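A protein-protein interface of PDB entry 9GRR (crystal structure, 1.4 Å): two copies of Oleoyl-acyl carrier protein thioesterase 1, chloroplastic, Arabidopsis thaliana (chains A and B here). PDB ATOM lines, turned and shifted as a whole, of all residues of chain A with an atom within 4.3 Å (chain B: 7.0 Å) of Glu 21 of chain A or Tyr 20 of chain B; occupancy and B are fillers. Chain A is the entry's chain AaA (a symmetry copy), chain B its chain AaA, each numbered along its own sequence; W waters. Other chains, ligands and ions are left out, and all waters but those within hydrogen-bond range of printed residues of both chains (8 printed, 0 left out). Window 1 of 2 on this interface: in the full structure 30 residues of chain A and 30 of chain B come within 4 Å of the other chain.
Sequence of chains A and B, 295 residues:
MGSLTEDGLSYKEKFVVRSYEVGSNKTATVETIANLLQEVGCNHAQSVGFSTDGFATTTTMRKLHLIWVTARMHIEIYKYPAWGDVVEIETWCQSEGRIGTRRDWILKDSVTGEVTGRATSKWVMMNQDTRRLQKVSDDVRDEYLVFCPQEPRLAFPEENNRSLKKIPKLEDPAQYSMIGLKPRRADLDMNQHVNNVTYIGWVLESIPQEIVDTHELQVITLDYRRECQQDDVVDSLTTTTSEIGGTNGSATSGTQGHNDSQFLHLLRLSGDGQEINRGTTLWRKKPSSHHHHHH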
ATOM      1  N   VAL A  16      33.455 -10.269   6.328  1.00  0.00           N
ATOM      2  CA  VAL A  16      32.848 -11.476   6.951  1.00  0.00           C
ATOM      3  C   VAL A  16      31.416 -11.558   6.444  1.00  0.00           C
ATOM      4  O   VAL A  16      30.661 -10.621   6.718  1.00  0.00           O
ATOM      5  CB  VAL A  16      32.934 -11.394   8.480  1.00  0.00           C
ATOM      6  CG1 VAL A  16      32.223 -12.577   9.091  1.00  0.00           C
ATOM      7  CG2 VAL A  16      34.389 -11.329   8.939  1.00  0.00           C
ATOM      8  N   VAL A  17      31.097 -12.597   5.691  1.00  0.00           N
ATOM      9  CA  VAL A  17      29.761 -12.737   5.028  1.00  0.00           C
ATOM     10  C   VAL A  17      28.670 -12.744   6.115  1.00  0.00           C
ATOM     11  O   VAL A  17      28.777 -13.525   7.113  1.00  0.00           O
ATOM     12  CB  VAL A  17      29.675 -13.961   4.106  1.00  0.00           C
ATOM     13  CG1 VAL A  17      28.305 -14.071   3.491  1.00  0.00           C
ATOM     14  CG2 VAL A  17      30.714 -13.930   2.989  1.00  0.00           C
ATOM     15  N   ARG A  18      27.681 -11.889   5.964  1.00  0.00           N
ATOM     16  CA  ARG A  18      26.611 -11.692   6.976  1.00  0.00           C
ATOM     17  C   ARG A  18      25.406 -12.571   6.641  1.00  0.00           C
ATOM     18  O   ARG A  18      25.237 -13.031   5.506  1.00  0.00           O
ATOM     19  CB  ARG A  18      26.211 -10.231   7.036  1.00  0.00           C
ATOM     20  CG  ARG A  18      27.312  -9.303   7.529  1.00  0.00           C
ATOM     21  CD  ARG A  18      26.954  -7.850   7.391  1.00  0.00           C
ATOM     22  NE  ARG A  18      28.045  -6.996   7.780  1.00  0.00           N
ATOM     23  CZ  ARG A  18      28.094  -5.660   7.616  1.00  0.00           C
ATOM     24  NH1 ARG A  18      27.064  -5.002   7.111  1.00  0.00           N
ATOM     25  NH2 ARG A  18      29.172  -4.989   7.993  1.00  0.00           N
ATOM     26  N   SER A  19      24.626 -12.886   7.683  1.00  0.00           N
ATOM     27  CA  SER A  19      23.456 -13.786   7.560  1.00  0.00           C
ATOM     28  C   SER A  19      22.505 -13.297   6.471  1.00  0.00           C
ATOM     29  O   SER A  19      22.016 -14.126   5.663  1.00  0.00           O
ATOM     30  CB  SER A  19      22.752 -13.897   8.925  1.00  0.00           C
ATOM     31  OG  SER A  19      22.171 -12.677   9.317  1.00  0.00           O
ATOM     32  N   TYR A  20      22.267 -11.994   6.436  1.00  0.00           N
ATOM     33  CA  TYR A  20      21.248 -11.408   5.545  1.00  0.00           C
ATOM     34  C   TYR A  20      21.807 -11.230   4.132  1.00  0.00           C
ATOM     35  O   TYR A  20      21.033 -10.937   3.218  1.00  0.00           O
ATOM     36  CB  TYR A  20      20.716 -10.084   6.061  1.00  0.00           C
ATOM     37  CG  TYR A  20      21.708  -8.963   6.175  1.00  0.00           C
ATOM     38  CD1 TYR A  20      22.002  -8.151   5.084  1.00  0.00           C
ATOM     39  CD2 TYR A  20      22.316  -8.649   7.370  1.00  0.00           C
ATOM     40  CE1 TYR A  20      22.846  -7.067   5.216  1.00  0.00           C
ATOM     41  CE2 TYR A  20      23.185  -7.595   7.508  1.00  0.00           C
ATOM     42  CZ  TYR A  20      23.471  -6.795   6.413  1.00  0.00           C
ATOM     43  OH  TYR A  20      24.336  -5.759   6.565  1.00  0.00           O
ATOM     44  N   GLU A  21      23.102 -11.446   3.955  1.00  0.00           N
ATOM     45  CA  GLU A  21      23.758 -11.367   2.618  1.00  0.00           C
ATOM     46  C   GLU A  21      23.648 -12.667   1.825  1.00  0.00           C
ATOM     47  O   GLU A  21      24.124 -12.713   0.673  1.00  0.00           O
ATOM     48  CB  GLU A  21      25.235 -10.991   2.795  1.00  0.00           C
ATOM     49  CG  GLU A  21      25.441  -9.549   3.197  1.00  0.00           C
ATOM     50  CD  GLU A  21      26.856  -9.125   3.569  1.00  0.00           C
ATOM     51  OE1 GLU A  21      27.693  -9.997   3.799  1.00  0.00           O
ATOM     52  OE2 GLU A  21      27.096  -7.882   3.629  1.00  0.00           O
ATOM     53  N   VAL A  22      23.150 -13.771   2.421  1.00  0.00           N
ATOM     54  CA  VAL A  22      23.176 -15.072   1.702  1.00  0.00           C
ATOM     55  C   VAL A  22      21.758 -15.459   1.265  1.00  0.00           C
ATOM     56  O   VAL A  22      20.797 -15.003   1.912  1.00  0.00           O
ATOM     57  CB  VAL A  22      23.888 -16.198   2.475  1.00  0.00           C
ATOM     58  CG1 VAL A  22      25.243 -15.739   3.018  1.00  0.00           C
ATOM     59  CG2 VAL A  22      23.004 -16.772   3.560  1.00  0.00           C
ATOM     60  N   ALA A  28      26.768 -16.309  -0.219  1.00  0.00           N
ATOM     61  CA  ALA A  28      26.544 -14.892  -0.589  1.00  0.00           C
ATOM     62  C   ALA A  28      25.861 -14.807  -1.951  1.00  0.00           C
ATOM     63  O   ALA A  28      26.260 -15.484  -2.887  1.00  0.00           O
ATOM     64  CB  ALA A  28      27.851 -14.144  -0.589  1.00  0.00           C
ATOM     65  N   THR A  29      24.896 -13.902  -2.068  1.00  0.00           N
ATOM     66  CA  THR A  29      24.255 -13.648  -3.386  1.00  0.00           C
ATOM     67  C   THR A  29      25.223 -12.889  -4.302  1.00  0.00           C
ATOM     68  O   THR A  29      26.146 -12.218  -3.801  1.00  0.00           O
ATOM     69  CB  THR A  29      22.962 -12.845  -3.244  1.00  0.00           C
ATOM     70  OG1 THR A  29      23.276 -11.551  -2.732  1.00  0.00           O
ATOM     71  CG2 THR A  29      21.996 -13.555  -2.315  1.00  0.00           C
ATOM     72  N   THR A  32      25.202  -9.343  -3.252  1.00  0.00           N
ATOM     73  CA  THR A  32      26.133  -9.050  -2.150  1.00  0.00           C
ATOM     74  C   THR A  32      27.527  -8.899  -2.763  1.00  0.00           C
ATOM     75  O   THR A  32      28.225  -7.938  -2.385  1.00  0.00           O
ATOM     76  CB  THR A  32      26.118 -10.160  -1.102  1.00  0.00           C
ATOM     77  OG1 THR A  32      24.851 -10.070  -0.438  1.00  0.00           O
ATOM     78  CG2 THR A  32      27.246 -10.023  -0.098  1.00  0.00           C
ATOM     79  N   ASN A  35      27.933  -5.548  -4.329  1.00  0.00           N
ATOM     80  CA  ASN A  35      28.036  -4.493  -3.321  1.00  0.00           C
ATOM     81  C   ASN A  35      29.451  -4.471  -2.745  1.00  0.00           C
ATOM     82  O   ASN A  35      29.971  -3.372  -2.502  1.00  0.00           O
ATOM     83  CB  ASN A  35      27.010  -4.698  -2.200  1.00  0.00           C
ATOM     84  CG  ASN A  35      25.628  -4.215  -2.562  1.00  0.00           C
ATOM     85  OD1 ASN A  35      24.638  -4.868  -2.180  1.00  0.00           O
ATOM     86  ND2 ASN A  35      25.541  -3.074  -3.186  1.00  0.00           N
ATOM     87  N   LEU A  36      30.014  -5.632  -2.437  1.00  0.00           N
ATOM     88  CA  LEU A  36      31.380  -5.678  -1.871  1.00  0.00           C
ATOM     89  C   LEU A  36      32.386  -5.134  -2.895  1.00  0.00           C
ATOM     90  O   LEU A  36      33.345  -4.429  -2.451  1.00  0.00           O
ATOM     91  CB  LEU A  36      31.765  -7.093  -1.452  1.00  0.00           C
ATOM     92  CG  LEU A  36      30.871  -7.745  -0.388  1.00  0.00           C
ATOM     93  CD1 LEU A  36      31.486  -9.080  -0.011  1.00  0.00           C
ATOM     94  CD2 LEU A  36      30.678  -6.840   0.797  1.00  0.00           C
ATOM     95  N   GLU A  39      32.126  -1.414  -2.612  1.00  0.00           N
ATOM     96  CA  GLU A  39      32.669  -0.930  -1.324  1.00  0.00           C
ATOM     97  C   GLU A  39      34.204  -0.885  -1.384  1.00  0.00           C
ATOM     98  O   GLU A  39      34.757   0.131  -0.964  1.00  0.00           O
ATOM     99  CB  GLU A  39      32.154  -1.807  -0.175  1.00  0.00           C
ATOM    100  CG  GLU A  39      32.812  -1.524   1.175  1.00  0.00           C
ATOM    101  CD  GLU A  39      32.545  -0.204   1.869  1.00  0.00           C
ATOM    102  OE1 GLU A  39      31.867   0.637   1.304  1.00  0.00           O
ATOM    103  OE2 GLU A  39      33.068  -0.016   2.987  1.00  0.00           O
ATOM    104  N   ASN A 195      21.382   2.661  -7.448  1.00  0.00           N
ATOM    105  CA  ASN A 195      22.614   1.855  -7.271  1.00  0.00           C
ATOM    106  C   ASN A 195      22.802   0.940  -8.474  1.00  0.00           C
ATOM    107  O   ASN A 195      21.819   0.259  -8.867  1.00  0.00           O
ATOM    108  CB  ASN A 195      22.470   1.011  -6.010  1.00  0.00           C
ATOM    109  CG  ASN A 195      23.736   0.308  -5.569  1.00  0.00           C
ATOM    110  OD1 ASN A 195      24.485  -0.246  -6.379  1.00  0.00           O
ATOM    111  ND2 ASN A 195      23.961   0.308  -4.265  1.00  0.00           N
ATOM    112  N   VAL B  17      30.526   1.156   8.856  1.00  0.00           N
ATOM    113  CA  VAL B  17      29.415   1.558   7.936  1.00  0.00           C
ATOM    114  C   VAL B  17      29.964   1.624   6.499  1.00  0.00           C
ATOM    115  O   VAL B  17      31.026   2.279   6.258  1.00  0.00           O
ATOM    116  CB  VAL B  17      28.730   2.865   8.360  1.00  0.00           C
ATOM    117  CG1 VAL B  17      27.644   3.239   7.386  1.00  0.00           C
ATOM    118  CG2 VAL B  17      28.129   2.787   9.760  1.00  0.00           C
ATOM    119  N   ARG B  18      29.304   0.945   5.584  1.00  0.00           N
ATOM    120  CA  ARG B  18      29.764   0.814   4.176  1.00  0.00           C
ATOM    121  C   ARG B  18      29.112   1.892   3.311  1.00  0.00           C
ATOM    122  O   ARG B  18      28.087   2.480   3.673  1.00  0.00           O
ATOM    123  CB  ARG B  18      29.439  -0.569   3.648  1.00  0.00           C
ATOM    124  CG  ARG B  18      30.185  -1.695   4.349  1.00  0.00           C
ATOM    125  CD  ARG B  18      29.700  -3.058   3.942  1.00  0.00           C
ATOM    126  NE  ARG B  18      30.358  -4.100   4.685  1.00  0.00           N
ATOM    127  CZ  ARG B  18      30.029  -5.405   4.667  1.00  0.00           C
ATOM    128  NH1 ARG B  18      29.062  -5.850   3.881  1.00  0.00           N
ATOM    129  NH2 ARG B  18      30.698  -6.265   5.421  1.00  0.00           N
ATOM    130  N   SER B  19      29.791   2.219   2.203  1.00  0.00           N
ATOM    131  CA  SER B  19      29.348   3.291   1.284  1.00  0.00           C
ATOM    132  C   SER B  19      27.910   3.059   0.827  1.00  0.00           C
ATOM    133  O   SER B  19      27.109   4.026   0.801  1.00  0.00           O
ATOM    134  CB  SER B  19      30.319   3.374   0.091  1.00  0.00           C
ATOM    135  OG  SER B  19      30.259   2.223  -0.716  1.00  0.00           O
ATOM    136  N   TYR B  20      27.588   1.816   0.501  1.00  0.00           N
ATOM    137  CA  TYR B  20      26.288   1.479  -0.109  1.00  0.00           C
ATOM    138  C   TYR B  20      25.206   1.357   0.966  1.00  0.00           C
ATOM    139  O   TYR B  20      24.026   1.274   0.616  1.00  0.00           O
ATOM    140  CB  TYR B  20      26.344   0.206  -0.933  1.00  0.00           C
ATOM    141  CG  TYR B  20      26.674  -1.057  -0.192  1.00  0.00           C
ATOM    142  CD1 TYR B  20      25.682  -1.794   0.449  1.00  0.00           C
ATOM    143  CD2 TYR B  20      27.950  -1.573  -0.168  1.00  0.00           C
ATOM    144  CE1 TYR B  20      25.976  -3.000   1.052  1.00  0.00           C
ATOM    145  CE2 TYR B  20      28.263  -2.754   0.459  1.00  0.00           C
ATOM    146  CZ  TYR B  20      27.267  -3.478   1.094  1.00  0.00           C
ATOM    147  OH  TYR B  20      27.594  -4.642   1.713  1.00  0.00           O
ATOM    148  N   GLU B  21      25.594   1.392   2.232  1.00  0.00           N
ATOM    149  CA  GLU B  21      24.635   1.346   3.372  1.00  0.00           C
ATOM    150  C   GLU B  21      24.069   2.718   3.728  1.00  0.00           C
ATOM    151  O   GLU B  21      23.223   2.804   4.641  1.00  0.00           O
ATOM    152  CB  GLU B  21      25.327   0.737   4.598  1.00  0.00           C
ATOM    153  CG  GLU B  21      25.557  -0.752   4.478  1.00  0.00           C
ATOM    154  CD  GLU B  21      26.394  -1.418   5.563  1.00  0.00           C
ATOM    155  OE1 GLU B  21      27.067  -0.708   6.310  1.00  0.00           O
ATOM    156  OE2 GLU B  21      26.357  -2.683   5.634  1.00  0.00           O
ATOM    157  N   VAL B  22      24.574   3.822   3.138  1.00  0.00           N
ATOM    158  CA  VAL B  22      24.130   5.168   3.586  1.00  0.00           C
ATOM    159  C   VAL B  22      23.228   5.804   2.521  1.00  0.00           C
ATOM    160  O   VAL B  22      23.361   5.436   1.340  1.00  0.00           O
ATOM    161  CB  VAL B  22      25.282   6.093   4.018  1.00  0.00           C
ATOM    162  CG1 VAL B  22      26.246   5.385   4.975  1.00  0.00           C
ATOM    163  CG2 VAL B  22      25.997   6.685   2.825  1.00  0.00           C
ATOM    164  N   GLY B  23      22.384   6.715   2.983  1.00  0.00           N
ATOM    165  CA  GLY B  23      21.439   7.497   2.155  1.00  0.00           C
ATOM    166  C   GLY B  23      21.964   8.898   1.894  1.00  0.00           C
ATOM    167  O   GLY B  23      23.187   9.091   1.971  1.00  0.00           O
ATOM    168  N   THR B  29      21.230   4.124   6.592  1.00  0.00           N
ATOM    169  CA  THR B  29      19.744   4.098   6.535  1.00  0.00           C
ATOM    170  C   THR B  29      19.187   3.295   7.717  1.00  0.00           C
ATOM    171  O   THR B  29      19.908   2.448   8.279  1.00  0.00           O
ATOM    172  CB  THR B  29      19.236   3.488   5.227  1.00  0.00           C
ATOM    173  OG1 THR B  29      19.630   2.118   5.174  1.00  0.00           O
ATOM    174  CG2 THR B  29      19.798   4.242   4.038  1.00  0.00           C
ATOM    175  N   THR B  32      19.596  -0.292   6.918  1.00  0.00           N
ATOM    176  CA  THR B  32      20.920  -0.827   7.274  1.00  0.00           C
ATOM    177  C   THR B  32      20.899  -1.126   8.775  1.00  0.00           C
ATOM    178  O   THR B  32      21.375  -2.213   9.157  1.00  0.00           O
ATOM    179  CB  THR B  32      22.030   0.166   6.934  1.00  0.00           C
ATOM    180  OG1 THR B  32      22.111   0.202   5.504  1.00  0.00           O
ATOM    181  CG2 THR B  32      23.366  -0.237   7.525  1.00  0.00           C
ATOM    182  N   GLU B  39      21.746  -9.196  12.146  1.00  0.00           N
ATOM    183  CA  GLU B  39      23.055  -9.878  12.056  1.00  0.00           C
ATOM    184  C   GLU B  39      23.606 -10.147  13.465  1.00  0.00           C
ATOM    185  O   GLU B  39      24.054 -11.271  13.692  1.00  0.00           O
ATOM    186  CB  GLU B  39      24.021  -9.050  11.198  1.00  0.00           C
ATOM    187  CG  GLU B  39      25.462  -9.558  11.206  1.00  0.00           C
ATOM    188  CD  GLU B  39      25.785 -10.884  10.549  1.00  0.00           C
ATOM    189  OE1 GLU B  39      24.877 -11.555  10.088  1.00  0.00           O
ATOM    190  OE2 GLU B  39      26.977 -11.256  10.539  1.00  0.00           O
ATOM    191  N   TRP B  83      29.381   6.768   6.757  1.00  0.00           N
ATOM    192  CA  TRP B  83      30.302   5.867   5.996  1.00  0.00           C
ATOM    193  C   TRP B  83      31.666   5.901   6.676  1.00  0.00           C
ATOM    194  O   TRP B  83      32.197   7.015   6.909  1.00  0.00           O
ATOM    195  CB  TRP B  83      30.440   6.255   4.502  1.00  0.00           C
ATOM    196  CG  TRP B  83      31.472   5.523   3.688  1.00  0.00           C
ATOM    197  CD1 TRP B  83      31.933   4.245   3.833  1.00  0.00           C
ATOM    198  CD2 TRP B  83      32.186   6.054   2.554  1.00  0.00           C
ATOM    199  NE1 TRP B  83      32.877   3.946   2.880  1.00  0.00           N
ATOM    200  CE2 TRP B  83      33.059   5.045   2.081  1.00  0.00           C
ATOM    201  CE3 TRP B  83      32.172   7.285   1.894  1.00  0.00           C
ATOM    202  CZ2 TRP B  83      33.900   5.233   0.982  1.00  0.00           C
ATOM    203  CZ3 TRP B  83      33.005   7.472   0.813  1.00  0.00           C
ATOM    204  CH2 TRP B  83      33.853   6.461   0.362  1.00  0.00           C
ATOM    205  N   MET B 190      17.672 -16.625   3.750  1.00  0.00           N
ATOM    206  CA  MET B 190      18.262 -17.929   3.361  1.00  0.00           C
ATOM    207  C   MET B 190      17.192 -19.033   3.407  1.00  0.00           C
ATOM    208  O   MET B 190      17.403 -20.089   2.774  1.00  0.00           O
ATOM    209  CB  MET B 190      19.468 -18.263   4.244  1.00  0.00           C
ATOM    210  CG  MET B 190      19.130 -18.588   5.687  1.00  0.00           C
ATOM    211  SD  MET B 190      20.639 -18.957   6.628  1.00  0.00           S
ATOM    212  CE  MET B 190      21.282 -17.308   6.916  1.00  0.00           C
ATOM    213  N   ASN B 195      12.474 -11.122   4.037  1.00  0.00           N
ATOM    214  CA  ASN B 195      13.248 -10.531   5.157  1.00  0.00           C
ATOM    215  C   ASN B 195      12.371  -9.542   5.915  1.00  0.00           C
ATOM    216  O   ASN B 195      11.726  -8.687   5.255  1.00  0.00           O
ATOM    217  CB  ASN B 195      14.457  -9.801   4.586  1.00  0.00           C
ATOM    218  CG  ASN B 195      15.466  -9.343   5.616  1.00  0.00           C
ATOM    219  OD1 ASN B 195      15.116  -8.831   6.683  1.00  0.00           O
ATOM    220  ND2 ASN B 195      16.736  -9.503   5.278  1.00  0.00           N
HETATM  221  O   HOH W   1      28.558  -2.208   8.054  1.00  0.00           O
HETATM  222  O   HOH W   2      32.885  -7.554   7.535  1.00  0.00           O
HETATM  223  O   HOH W   3      24.560  -4.160   4.499  1.00  0.00           O
HETATM  224  O   HOH W   4      18.059 -11.546   3.962  1.00  0.00           O
HETATM  225  O   HOH W   5      19.449 -14.635   4.941  1.00  0.00           O
HETATM  226  O   HOH W   6      25.574  -6.048   2.618  1.00  0.00           O
HETATM  227  O   HOH W   7      30.092  -8.914   4.570  1.00  0.00           O
HETATM  228  O   HOH W   8      23.604   2.247  -2.324  1.00  0.00           O
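OE1 of Glu 39 of chain B is in hydrogen-bond range of N of Ser 19 of chain A (2.8 Å).
The side-chain carboxylate of Glu 39 of chain A sits at hydrogen-bond distance from the backbone NH of Ser 19 of chain B (2.8 Å).
NH1 of Arg 18 of chain A lies within salt-bridge range of OE2 of Glu 21 of chain B (2.8 Å).
OE2 of Glu 21 of chain A lies within salt-bridge range of NH1 of Arg 18 of chain B (2.8 Å).
The guanidinium group of Arg 18 of chain B sits close to the guanidinium group of Arg 18 of chain A, at 3.3 Å.
The backbone carbonyl oxygen (O) of Glu 21 of chain A sits at hydrogen-bond distance from the side-chain hydroxyl (OG1) of Thr 32 of chain A, at 3.0 Å.
The guanidinium group of Arg 18 of chain B lies within hydrogen-bond range of the side-chain hydroxyl of Tyr 20 of chain B (2.9 Å).
The guanidinium group of Arg 18 of chain A sits at hydrogen-bond distance from the side-chain hydroxyl of Tyr 20 of chain A.
The backbone NH (N) of Arg 18 of chain B lies within hydrogen-bond range of the side-chain carboxylate (OE1) of Glu 21 of chain B (2.9 Å).
The backbone carbonyl oxygen (O) of Glu 21 of chain B sits at hydrogen-bond distance from the side-chain hydroxyl (OG1) of Thr 32 of chain B.
The backbone carbonyl oxygen of Glu 21 of chain A is in hydrogen-bond range of the backbone NH of Thr 29 of chain A (3.1 Å).
Glu 39 of chain B touches Arg 18 of chain A (OE1 to CA, 3.6 Å).
Ser 19 of chain A touches Met 190 of chain B.
OE2 of Glu 21 of chain B touches OH of Tyr 20 of chain A, 3.8 Å away.
OE2 of Glu 21 of chain A touches OH of Tyr 20 of chain B, at 3.8 Å.
CE of Met 190 of chain B touches CG2 of Val 22 of chain A, 3.8 Å away.
Asn 35 of chain A touches Tyr 20 of chain B (O to CE2, 3.5 Å).
Leu 36 of chain A touches Arg 18 of chain B.
Tyr 20 of chain B touches Leu 36 of chain A.
Glu 39 of chain A touches Arg 18 of chain B (OE1 to CA, 3.6 Å).
Glu 39 of chain A touches Trp 83 of chain B (OE1 to NE1, 3.8 Å).
Of the printed residues of chain B, Ser 19 of chain A touches Glu 39 and Met 190.
Of chain B, only Arg 18 (2.8 Å) and Tyr 20 (3.8 Å) come within 4 Å of Glu 21 of chain A.
Printed residues of chain B within 4 Å of Asn 35 of chain A: Tyr 20 (3.5 Å).
Of the printed residues of chain A, Glu 39 of chain B touches Arg 18 and Ser 19.
The nearest residue of chain A that does not touch Tyr 20 of chain B is Glu 39 of chain A (4.1 Å).
Hydrophobic or aromatic side chains of chain A that line the printed part of chain B: Tyr 20, Val 22 and Leu 36.
Among the printed residues, 15 pairs touch across the chains.
Arg 18 of chain B touches its own counterpart, Arg 18 of chain A.
Arg 18 of chain A touches Glu 21 of chain B, and with the chains exchanged Glu 21 of chain A touches Arg 18 of chain B.
Ser 19 of chain A touches Glu 39 of chain B, and with the chains exchanged Glu 39 of chain A touches Ser 19 of chain B.
Tyr 20 of chain A touches Glu 21 of chain B, and with the chains exchanged Glu 21 of chain A touches Tyr 20 of chain B.
Of the 15 pairs that touch across the chains among the printed residues, 9 have their exchanged pair printed and touching as well.
Water W3 lies within hydrogen-bond range of the side-chain carboxylate of Glu 21 of chain B (2.6 Å) and the side-chain hydroxyl of Tyr 20 of chain A (2.6 Å).
Water W5 lies within hydrogen-bond range of the backbone carbonyl oxygen (O) of Ser 19 of chain A (2.7 Å), the backbone NH (N) of Met 190 of chain B (2.9 Å) and the backbone carbonyl oxygen (O) of Val 22 of chain A (3.3 Å).
Water W7 lies within hydrogen-bond range of OE1 of Glu 21 of chain A (2.7 Å), O of Val 16 of chain A (2.8 Å) and NH2 of Arg 18 of chain B (2.8 Å).
Water W1 bridges the side-chain carboxylate (OE1) of Glu 21 of chain B (2.7 Å) and the guanidinium group (NH2) of Arg 18 of chain A (2.8 Å).
Water W8 lies within hydrogen-bond range of the side-chain amide nitrogen (ND2) of Asn 195 of chain A (2.8 Å) and the backbone carbonyl oxygen (O) of Tyr 20 of chain B (3.1 Å).
Water W2 lies within hydrogen-bond range of N of Val 16 of chain A (3.0 Å) and NH2 of Arg 18 of chain B (3.3 Å).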
